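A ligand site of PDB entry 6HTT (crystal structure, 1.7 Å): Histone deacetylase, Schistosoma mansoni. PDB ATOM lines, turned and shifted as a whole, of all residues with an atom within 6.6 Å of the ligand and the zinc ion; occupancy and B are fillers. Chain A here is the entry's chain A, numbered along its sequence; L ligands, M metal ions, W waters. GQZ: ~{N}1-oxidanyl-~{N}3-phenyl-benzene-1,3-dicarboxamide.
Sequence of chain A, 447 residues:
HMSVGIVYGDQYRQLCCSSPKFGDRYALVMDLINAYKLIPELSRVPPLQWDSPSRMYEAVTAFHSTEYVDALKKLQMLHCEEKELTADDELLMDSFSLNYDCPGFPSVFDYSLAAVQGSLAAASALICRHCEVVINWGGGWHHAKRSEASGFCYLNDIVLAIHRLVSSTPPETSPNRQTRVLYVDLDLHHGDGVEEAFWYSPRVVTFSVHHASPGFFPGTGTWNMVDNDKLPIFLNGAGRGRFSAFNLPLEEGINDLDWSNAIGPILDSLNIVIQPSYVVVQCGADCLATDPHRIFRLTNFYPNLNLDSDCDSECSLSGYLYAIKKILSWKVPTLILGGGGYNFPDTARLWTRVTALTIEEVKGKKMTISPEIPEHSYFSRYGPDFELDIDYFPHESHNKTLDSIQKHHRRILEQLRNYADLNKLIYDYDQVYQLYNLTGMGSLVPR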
ATOM      1  N   LYS A  21      18.636   9.197  32.618  1.00  0.00           N
ATOM      2  CA  LYS A  21      17.566   9.418  31.654  1.00  0.00           C
ATOM      3  C   LYS A  21      16.269   9.850  32.336  1.00  0.00           C
ATOM      4  O   LYS A  21      15.562  10.733  31.835  1.00  0.00           O
ATOM      5  CB  LYS A  21      17.322   8.154  30.825  1.00  0.00           C
ATOM      6  CG  LYS A  21      16.354   8.418  29.667  1.00  0.00           C
ATOM      7  CD  LYS A  21      16.611   7.516  28.476  1.00  0.00           C
ATOM      8  CE  LYS A  21      15.885   8.028  27.231  1.00  0.00           C
ATOM      9  NZ  LYS A  21      16.269   9.430  26.866  1.00  0.00           N
ATOM     10  N   PHE A  22      15.928   9.236  33.471  1.00  0.00           N
ATOM     11  CA  PHE A  22      14.631   9.520  34.083  1.00  0.00           C
ATOM     12  C   PHE A  22      14.739  10.460  35.279  1.00  0.00           C
ATOM     13  O   PHE A  22      13.703  10.841  35.827  1.00  0.00           O
ATOM     14  CB  PHE A  22      13.923   8.212  34.446  1.00  0.00           C
ATOM     15  CG  PHE A  22      13.424   7.479  33.223  1.00  0.00           C
ATOM     16  CD1 PHE A  22      12.259   7.895  32.588  1.00  0.00           C
ATOM     17  CD2 PHE A  22      14.155   6.442  32.659  1.00  0.00           C
ATOM     18  CE1 PHE A  22      11.808   7.247  31.433  1.00  0.00           C
ATOM     19  CE2 PHE A  22      13.712   5.800  31.507  1.00  0.00           C
ATOM     20  CZ  PHE A  22      12.535   6.206  30.899  1.00  0.00           C
ATOM     21  N   ASP A 101      22.503   3.922  24.045  1.00  0.00           N
ATOM     22  CA  ASP A 101      21.319   4.413  24.760  1.00  0.00           C
ATOM     23  C   ASP A 101      21.047   3.672  26.061  1.00  0.00           C
ATOM     24  O   ASP A 101      20.142   4.073  26.793  1.00  0.00           O
ATOM     25  CB  ASP A 101      20.083   4.344  23.858  1.00  0.00           C
ATOM     26  CG  ASP A 101      20.014   5.495  22.869  1.00  0.00           C
ATOM     27  OD1 ASP A 101      20.994   6.262  22.799  1.00  0.00           O
ATOM     28  OD2 ASP A 101      18.979   5.635  22.175  1.00  0.00           O
ATOM     29  N   GLY A 140       7.712  -1.056  34.734  1.00  0.00           N
ATOM     30  CA  GLY A 140       7.202  -1.016  33.376  1.00  0.00           C
ATOM     31  C   GLY A 140       8.237  -0.983  32.271  1.00  0.00           C
ATOM     32  O   GLY A 140       7.969  -0.393  31.212  1.00  0.00           O
ATOM     33  N   HIS A 142       9.673  -2.368  29.438  1.00  0.00           N
ATOM     34  CA  HIS A 142       9.204  -3.438  28.572  1.00  0.00           C
ATOM     35  C   HIS A 142      10.191  -3.855  27.483  1.00  0.00           C
ATOM     36  O   HIS A 142       9.957  -4.866  26.831  1.00  0.00           O
ATOM     37  CB  HIS A 142       7.847  -3.054  27.927  1.00  0.00           C
ATOM     38  CG  HIS A 142       7.866  -1.778  27.139  1.00  0.00           C
ATOM     39  ND1 HIS A 142       6.779  -1.351  26.404  1.00  0.00           N
ATOM     40  CD2 HIS A 142       8.806  -0.815  26.997  1.00  0.00           C
ATOM     41  CE1 HIS A 142       7.058  -0.198  25.819  1.00  0.00           C
ATOM     42  NE2 HIS A 142       8.287   0.156  26.167  1.00  0.00           N
ATOM     43  N   HIS A 143      11.301  -3.138  27.292  1.00  0.00           N
ATOM     44  CA  HIS A 143      12.197  -3.434  26.155  1.00  0.00           C
ATOM     45  C   HIS A 143      13.304  -4.436  26.472  1.00  0.00           C
ATOM     46  O   HIS A 143      13.894  -4.981  25.536  1.00  0.00           O
ATOM     47  CB  HIS A 143      12.859  -2.157  25.650  1.00  0.00           C
ATOM     48  CG  HIS A 143      11.913  -1.199  25.003  1.00  0.00           C
ATOM     49  ND1 HIS A 143      11.020  -1.584  24.026  1.00  0.00           N
ATOM     50  CD2 HIS A 143      11.735   0.140  25.174  1.00  0.00           C
ATOM     51  CE1 HIS A 143      10.335  -0.524  23.622  1.00  0.00           C
ATOM     52  NE2 HIS A 143      10.752   0.525  24.294  1.00  0.00           N
ATOM     53  N   SER A 150      17.913  -2.583  26.270  1.00  0.00           N
ATOM     54  CA  SER A 150      17.359  -1.929  25.088  1.00  0.00           C
ATOM     55  C   SER A 150      16.501  -0.759  25.550  1.00  0.00           C
ATOM     56  O   SER A 150      15.708  -0.906  26.470  1.00  0.00           O
ATOM     57  CB  SER A 150      16.529  -2.910  24.276  1.00  0.00           C
ATOM     58  OG  SER A 150      15.911  -2.244  23.168  1.00  0.00           O
ATOM     59  N   GLY A 151      16.652   0.387  24.885  1.00  0.00           N
ATOM     60  CA  GLY A 151      15.736   1.494  25.148  1.00  0.00           C
ATOM     61  C   GLY A 151      15.699   1.954  26.597  1.00  0.00           C
ATOM     62  O   GLY A 151      14.619   2.227  27.135  1.00  0.00           O
ATOM     63  N   PHE A 152      16.868   2.042  27.238  1.00  0.00           N
ATOM     64  CA  PHE A 152      17.052   2.368  28.659  1.00  0.00           C
ATOM     65  C   PHE A 152      16.295   1.422  29.592  1.00  0.00           C
ATOM     66  O   PHE A 152      16.024   1.776  30.751  1.00  0.00           O
ATOM     67  CB  PHE A 152      16.686   3.825  28.982  1.00  0.00           C
ATOM     68  CG  PHE A 152      17.472   4.375  30.159  1.00  0.00           C
ATOM     69  CD1 PHE A 152      18.773   4.797  29.986  1.00  0.00           C
ATOM     70  CD2 PHE A 152      16.916   4.410  31.441  1.00  0.00           C
ATOM     71  CE1 PHE A 152      19.525   5.273  31.058  1.00  0.00           C
ATOM     72  CE2 PHE A 152      17.646   4.882  32.509  1.00  0.00           C
ATOM     73  CZ  PHE A 152      18.959   5.327  32.320  1.00  0.00           C
ATOM     74  N   CYS A 153      15.998   0.221  29.110  1.00  0.00           N
ATOM     75  CA  CYS A 153      15.465  -0.868  29.922  1.00  0.00           C
ATOM     76  C   CYS A 153      16.570  -1.881  30.125  1.00  0.00           C
ATOM     77  O   CYS A 153      17.094  -2.425  29.139  1.00  0.00           O
ATOM     78  CB  CYS A 153      14.252  -1.526  29.232  1.00  0.00           C
ATOM     79  SG  CYS A 153      12.863  -0.411  28.942  1.00  0.00           S
ATOM     80  N   ASP A 187       2.115   2.042  26.092  1.00  0.00           N
ATOM     81  CA  ASP A 187       3.246   2.904  25.780  1.00  0.00           C
ATOM     82  C   ASP A 187       3.215   3.308  24.302  1.00  0.00           C
ATOM     83  O   ASP A 187       2.636   2.618  23.450  1.00  0.00           O
ATOM     84  CB  ASP A 187       4.544   2.158  26.095  1.00  0.00           C
ATOM     85  CG  ASP A 187       5.753   3.055  26.206  1.00  0.00           C
ATOM     86  OD1 ASP A 187       6.345   3.391  25.161  1.00  0.00           O
ATOM     87  OD2 ASP A 187       6.152   3.351  27.348  1.00  0.00           O
ATOM     88  N   LEU A 188       3.846   4.443  24.007  1.00  0.00           N
ATOM     89  CA  LEU A 188       4.016   4.859  22.609  1.00  0.00           C
ATOM     90  C   LEU A 188       4.776   3.825  21.805  1.00  0.00           C
ATOM     91  O   LEU A 188       4.582   3.698  20.602  1.00  0.00           O
ATOM     92  CB  LEU A 188       4.756   6.196  22.559  1.00  0.00           C
ATOM     93  CG  LEU A 188       5.014   6.766  21.163  1.00  0.00           C
ATOM     94  CD1 LEU A 188       3.709   7.189  20.499  1.00  0.00           C
ATOM     95  CD2 LEU A 188       5.972   7.949  21.266  1.00  0.00           C
ATOM     96  N   HIS A 189       5.651   3.077  22.459  1.00  0.00           N
ATOM     97  CA  HIS A 189       6.522   2.123  21.793  1.00  0.00           C
ATOM     98  C   HIS A 189       5.998   0.697  21.912  1.00  0.00           C
ATOM     99  O   HIS A 189       5.338   0.336  22.893  1.00  0.00           O
ATOM    100  CB  HIS A 189       7.939   2.187  22.373  1.00  0.00           C
ATOM    101  CG  HIS A 189       8.581   3.528  22.189  1.00  0.00           C
ATOM    102  ND1 HIS A 189       8.484   4.533  23.131  1.00  0.00           N
ATOM    103  CD2 HIS A 189       9.258   4.054  21.149  1.00  0.00           C
ATOM    104  CE1 HIS A 189       9.117   5.611  22.687  1.00  0.00           C
ATOM    105  NE2 HIS A 189       9.601   5.344  21.477  1.00  0.00           N
ATOM    106  N   HIS A 190       6.333  -0.114  20.906  1.00  0.00           N
ATOM    107  CA  HIS A 190       6.006  -1.539  20.939  1.00  0.00           C
ATOM    108  C   HIS A 190       6.654  -2.222  22.141  1.00  0.00           C
ATOM    109  O   HIS A 190       7.856  -2.074  22.397  1.00  0.00           O
ATOM    110  CB  HIS A 190       6.471  -2.194  19.646  1.00  0.00           C
ATOM    111  CG  HIS A 190       6.229  -3.679  19.612  1.00  0.00           C
ATOM    112  ND1 HIS A 190       7.227  -4.585  19.336  1.00  0.00           N
ATOM    113  CD2 HIS A 190       5.118  -4.399  19.874  1.00  0.00           C
ATOM    114  CE1 HIS A 190       6.733  -5.811  19.393  1.00  0.00           C
ATOM    115  NE2 HIS A 190       5.453  -5.734  19.726  1.00  0.00           N
ATOM    116  N   PHE A 217      11.751   3.457  16.773  1.00  0.00           N
ATOM    117  CA  PHE A 217      12.128   2.425  17.749  1.00  0.00           C
ATOM    118  C   PHE A 217      10.906   1.652  18.274  1.00  0.00           C
ATOM    119  O   PHE A 217       9.859   2.259  18.525  1.00  0.00           O
ATOM    120  CB  PHE A 217      12.881   3.113  18.899  1.00  0.00           C
ATOM    121  CG  PHE A 217      13.432   2.174  19.922  1.00  0.00           C
ATOM    122  CD1 PHE A 217      12.692   1.811  21.035  1.00  0.00           C
ATOM    123  CD2 PHE A 217      14.717   1.656  19.777  1.00  0.00           C
ATOM    124  CE1 PHE A 217      13.212   0.938  21.980  1.00  0.00           C
ATOM    125  CE2 PHE A 217      15.245   0.789  20.724  1.00  0.00           C
ATOM    126  CZ  PHE A 217      14.492   0.430  21.825  1.00  0.00           C
ATOM    127  N   GLN A 282       0.974  -1.822  31.131  1.00  0.00           N
ATOM    128  CA  GLN A 282       2.069  -0.868  31.060  1.00  0.00           C
ATOM    129  C   GLN A 282       1.457   0.448  30.608  1.00  0.00           C
ATOM    130  O   GLN A 282       0.773   0.499  29.574  1.00  0.00           O
ATOM    131  CB  GLN A 282       3.154  -1.390  30.103  1.00  0.00           C
ATOM    132  CG  GLN A 282       4.505  -0.725  30.243  1.00  0.00           C
ATOM    133  CD  GLN A 282       4.662   0.482  29.354  1.00  0.00           C
ATOM    134  OE1 GLN A 282       3.670   1.060  28.926  1.00  0.00           O
ATOM    135  NE2 GLN A 282       5.905   0.863  29.076  1.00  0.00           N
ATOM    136  N   GLY A 284       2.955   3.588  29.972  1.00  0.00           N
ATOM    137  CA  GLY A 284       3.900   4.601  29.541  1.00  0.00           C
ATOM    138  C   GLY A 284       3.198   5.851  29.038  1.00  0.00           C
ATOM    139  O   GLY A 284       2.264   5.768  28.247  1.00  0.00           O
ATOM    140  N   ASP A 286       4.290   8.341  27.172  1.00  0.00           N
ATOM    141  CA  ASP A 286       4.862   9.040  26.029  1.00  0.00           C
ATOM    142  C   ASP A 286       3.893   9.192  24.856  1.00  0.00           C
ATOM    143  O   ASP A 286       4.291   9.733  23.821  1.00  0.00           O
ATOM    144  CB  ASP A 286       6.174   8.377  25.533  1.00  0.00           C
ATOM    145  CG  ASP A 286       6.176   6.859  25.650  1.00  0.00           C
ATOM    146  OD1 ASP A 286       5.116   6.217  25.879  1.00  0.00           O
ATOM    147  OD2 ASP A 286       7.289   6.313  25.468  1.00  0.00           O
ATOM    148  N   ASP A 291       4.391  15.046  25.240  1.00  0.00           N
ATOM    149  CA  ASP A 291       5.644  14.310  25.337  1.00  0.00           C
ATOM    150  C   ASP A 291       6.616  14.821  24.276  1.00  0.00           C
ATOM    151  O   ASP A 291       6.196  15.185  23.176  1.00  0.00           O
ATOM    152  CB  ASP A 291       5.402  12.817  25.170  1.00  0.00           C
ATOM    153  CG  ASP A 291       6.622  12.011  25.518  1.00  0.00           C
ATOM    154  OD1 ASP A 291       7.487  11.848  24.629  1.00  0.00           O
ATOM    155  OD2 ASP A 291       6.736  11.589  26.700  1.00  0.00           O
ATOM    156  N   PRO A 292       7.920  14.870  24.574  1.00  0.00           N
ATOM    157  CA  PRO A 292       8.889  15.339  23.557  1.00  0.00           C
ATOM    158  C   PRO A 292       8.924  14.485  22.290  1.00  0.00           C
ATOM    159  O   PRO A 292       9.373  14.977  21.246  1.00  0.00           O
ATOM    160  CB  PRO A 292      10.237  15.298  24.277  1.00  0.00           C
ATOM    161  CG  PRO A 292       9.963  14.978  25.704  1.00  0.00           C
ATOM    162  CD  PRO A 292       8.543  14.578  25.883  1.00  0.00           C
ATOM    163  N   HIS A 293       8.454  13.227  22.346  1.00  0.00           N
ATOM    164  CA  HIS A 293       8.303  12.456  21.116  1.00  0.00           C
ATOM    165  C   HIS A 293       7.381  13.152  20.123  1.00  0.00           C
ATOM    166  O   HIS A 293       7.609  13.094  18.905  1.00  0.00           O
ATOM    167  CB  HIS A 293       7.763  11.075  21.431  1.00  0.00           C
ATOM    168  CG  HIS A 293       8.807  10.121  21.919  1.00  0.00           C
ATOM    169  ND1 HIS A 293       9.659   9.459  21.054  1.00  0.00           N
ATOM    170  CD2 HIS A 293       9.154   9.724  23.167  1.00  0.00           C
ATOM    171  CE1 HIS A 293      10.483   8.696  21.760  1.00  0.00           C
ATOM    172  NE2 HIS A 293      10.194   8.832  23.041  1.00  0.00           N
ATOM    173  N   GLY A 339       6.490   3.275  32.748  1.00  0.00           N
ATOM    174  CA  GLY A 339       7.198   3.065  31.485  1.00  0.00           C
ATOM    175  C   GLY A 339       7.728   4.407  30.959  1.00  0.00           C
ATOM    176  O   GLY A 339       8.216   5.230  31.724  1.00  0.00           O
ATOM    177  N   GLY A 340       7.629   4.579  29.645  1.00  0.00           N
ATOM    178  CA  GLY A 340       8.068   5.829  29.044  1.00  0.00           C
ATOM    179  C   GLY A 340       7.285   7.016  29.569  1.00  0.00           C
ATOM    180  O   GLY A 340       6.292   6.912  30.284  1.00  0.00           O
ATOM    181  N   GLY A 341       7.761   8.200  29.179  1.00  0.00           N
ATOM    182  CA  GLY A 341       7.176   9.465  29.588  1.00  0.00           C
ATOM    183  C   GLY A 341       8.277  10.463  29.891  1.00  0.00           C
ATOM    184  O   GLY A 341       8.883  10.403  30.964  1.00  0.00           O
ATOM    185  N   TYR A 342       8.552  11.371  28.968  1.00  0.00           N
ATOM    186  CA  TYR A 342       9.762  12.182  29.026  1.00  0.00           C
ATOM    187  C   TYR A 342       9.446  13.641  29.295  1.00  0.00           C
ATOM    188  O   TYR A 342      10.374  14.451  29.417  1.00  0.00           O
ATOM    189  CB  TYR A 342      10.564  11.957  27.734  1.00  0.00           C
ATOM    190  CG  TYR A 342      10.785  10.461  27.610  1.00  0.00           C
ATOM    191  CD1 TYR A 342      11.804   9.845  28.321  1.00  0.00           C
ATOM    192  CD2 TYR A 342       9.901   9.662  26.885  1.00  0.00           C
ATOM    193  CE1 TYR A 342      11.968   8.467  28.276  1.00  0.00           C
ATOM    194  CE2 TYR A 342      10.054   8.300  26.841  1.00  0.00           C
ATOM    195  CZ  TYR A 342      11.098   7.704  27.538  1.00  0.00           C
ATOM    196  OH  TYR A 342      11.260   6.349  27.485  1.00  0.00           O
HETATM  197  C10 GQZ L   1      11.957   4.886  24.530  1.00  0.00           C
HETATM  198  C11 GQZ L   1      12.290   6.239  24.539  1.00  0.00           C
HETATM  199  C12 GQZ L   1      13.465   6.690  23.945  1.00  0.00           C
HETATM  200  C13 GQZ L   1      14.314   5.769  23.321  1.00  0.00           C
HETATM  201  C14 GQZ L   1      13.991   4.423  23.305  1.00  0.00           C
HETATM  202  C15 GQZ L   1      10.689   4.426  25.171  1.00  0.00           C
HETATM  203  O17 GQZ L   1       9.204   2.679  25.645  1.00  0.00           O
HETATM  204  C1  GQZ L   1      13.424  10.998  25.275  1.00  0.00           C
HETATM  205  C2  GQZ L   1      12.959  10.427  24.098  1.00  0.00           C
HETATM  206  C3  GQZ L   1      12.603  11.252  23.037  1.00  0.00           C
HETATM  207  C4  GQZ L   1      12.703  12.627  23.159  1.00  0.00           C
HETATM  208  C5  GQZ L   1      13.152  13.186  24.332  1.00  0.00           C
HETATM  209  C6  GQZ L   1      13.511  12.376  25.385  1.00  0.00           C
HETATM  210  N7  GQZ L   1      12.841   9.025  23.980  1.00  0.00           N
HETATM  211  C8  GQZ L   1      13.849   8.130  24.053  1.00  0.00           C
HETATM  212  C9  GQZ L   1      12.830   3.982  23.912  1.00  0.00           C
HETATM  213  N16 GQZ L   1      10.381   3.144  25.053  1.00  0.00           N
HETATM  214  O18 GQZ L   1      15.023   8.460  24.227  1.00  0.00           O
HETATM  215  O19 GQZ L   1       9.959   5.212  25.774  1.00  0.00           O
HETATM  216 ZN    ZN M   1       7.989   4.481  25.183  1.00  0.00          ZN
HETATM  217  O   HOH W   1       9.707   2.334  28.386  1.00  0.00           O
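CA of Gly 151 touches C14 of the ligand, at 3.9 Å.
Phe 217 touches the ligand (CD1 to C9, 3.6 Å).
CB of Pro 292 touches C5 of the ligand (3.6 Å).
CA of Gly 340 touches O19 of the ligand (3.8 Å).
12 residues have an atom within 4 Å of the ligand: Lys 21, His 142, His 143, Gly 151, Asp 187, His 189, Phe 217, Asp 286, Pro 292, His 293, Gly 340 and Tyr 342.
The side-chain sulfur (SG) of Cys 153 is in hydrogen-bond range of the backbone carbonyl oxygen (O) of Gly 151 (3.6 Å).
A ring nitrogen (NE2) of His 142 sits at hydrogen-bond distance from a ring nitrogen (NE2) of His 143, 3.1 Å away.
The backbone NH of His 142 lies within hydrogen-bond range of the side-chain sulfur of Cys 153 (3.8 Å).
The backbone NH of His 293 is in hydrogen-bond range of the side-chain carboxylate of Asp 291, at 2.8 Å.
The side-chain carboxylate (OD2) of Asp 187 is in hydrogen-bond range of the side-chain amide nitrogen (NE2) of Gln 282.
OD2 of Asp 187 sits at hydrogen-bond distance from N of Gly 340, 3.0 Å away.
N of Tyr 342 is in hydrogen-bond range of OD2 of Asp 291, 2.9 Å away.
The side-chain carboxylate (OD1) of Asp 286 lies within hydrogen-bond range of the backbone NH (N) of Leu 188, 2.9 Å away.
The zinc ion is bound by the side-chain carboxylate (OD1) of Asp 187 (2.0 Å), the side-chain carboxylate (OD2) of Asp 286 (2.0 Å), a ring nitrogen (ND1) of His 189 (2.1 Å), an oxygen (O19) of the ligand (2.2 Å) and an oxygen (O17) of the ligand (2.2 Å).
Within 4 Å of the zinc ion: Asp 187, His 189 and Asp 286.
A nitrogen (N7) of the ligand sits at hydrogen-bond distance from a ring nitrogen (NE2) of His 293 (2.8 Å).
The side-chain amino group of Lys 21 sits at hydrogen-bond distance from an oxygen (O18) of the ligand, at 3.1 Å.
An oxygen (O17) of the ligand sits close to a ring nitrogen (NE2) of His 142.
A ring nitrogen (NE2) of His 143 lies within hydrogen-bond range of a nitrogen (N16) of the ligand.
OH of Tyr 342 sits close to O19 of the ligand (2.4 Å).
Water W1 lies within hydrogen-bond range of the backbone NH of Gly 340, a ring nitrogen (NE2) of His 142 and a nitrogen (N16) of the ligand.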
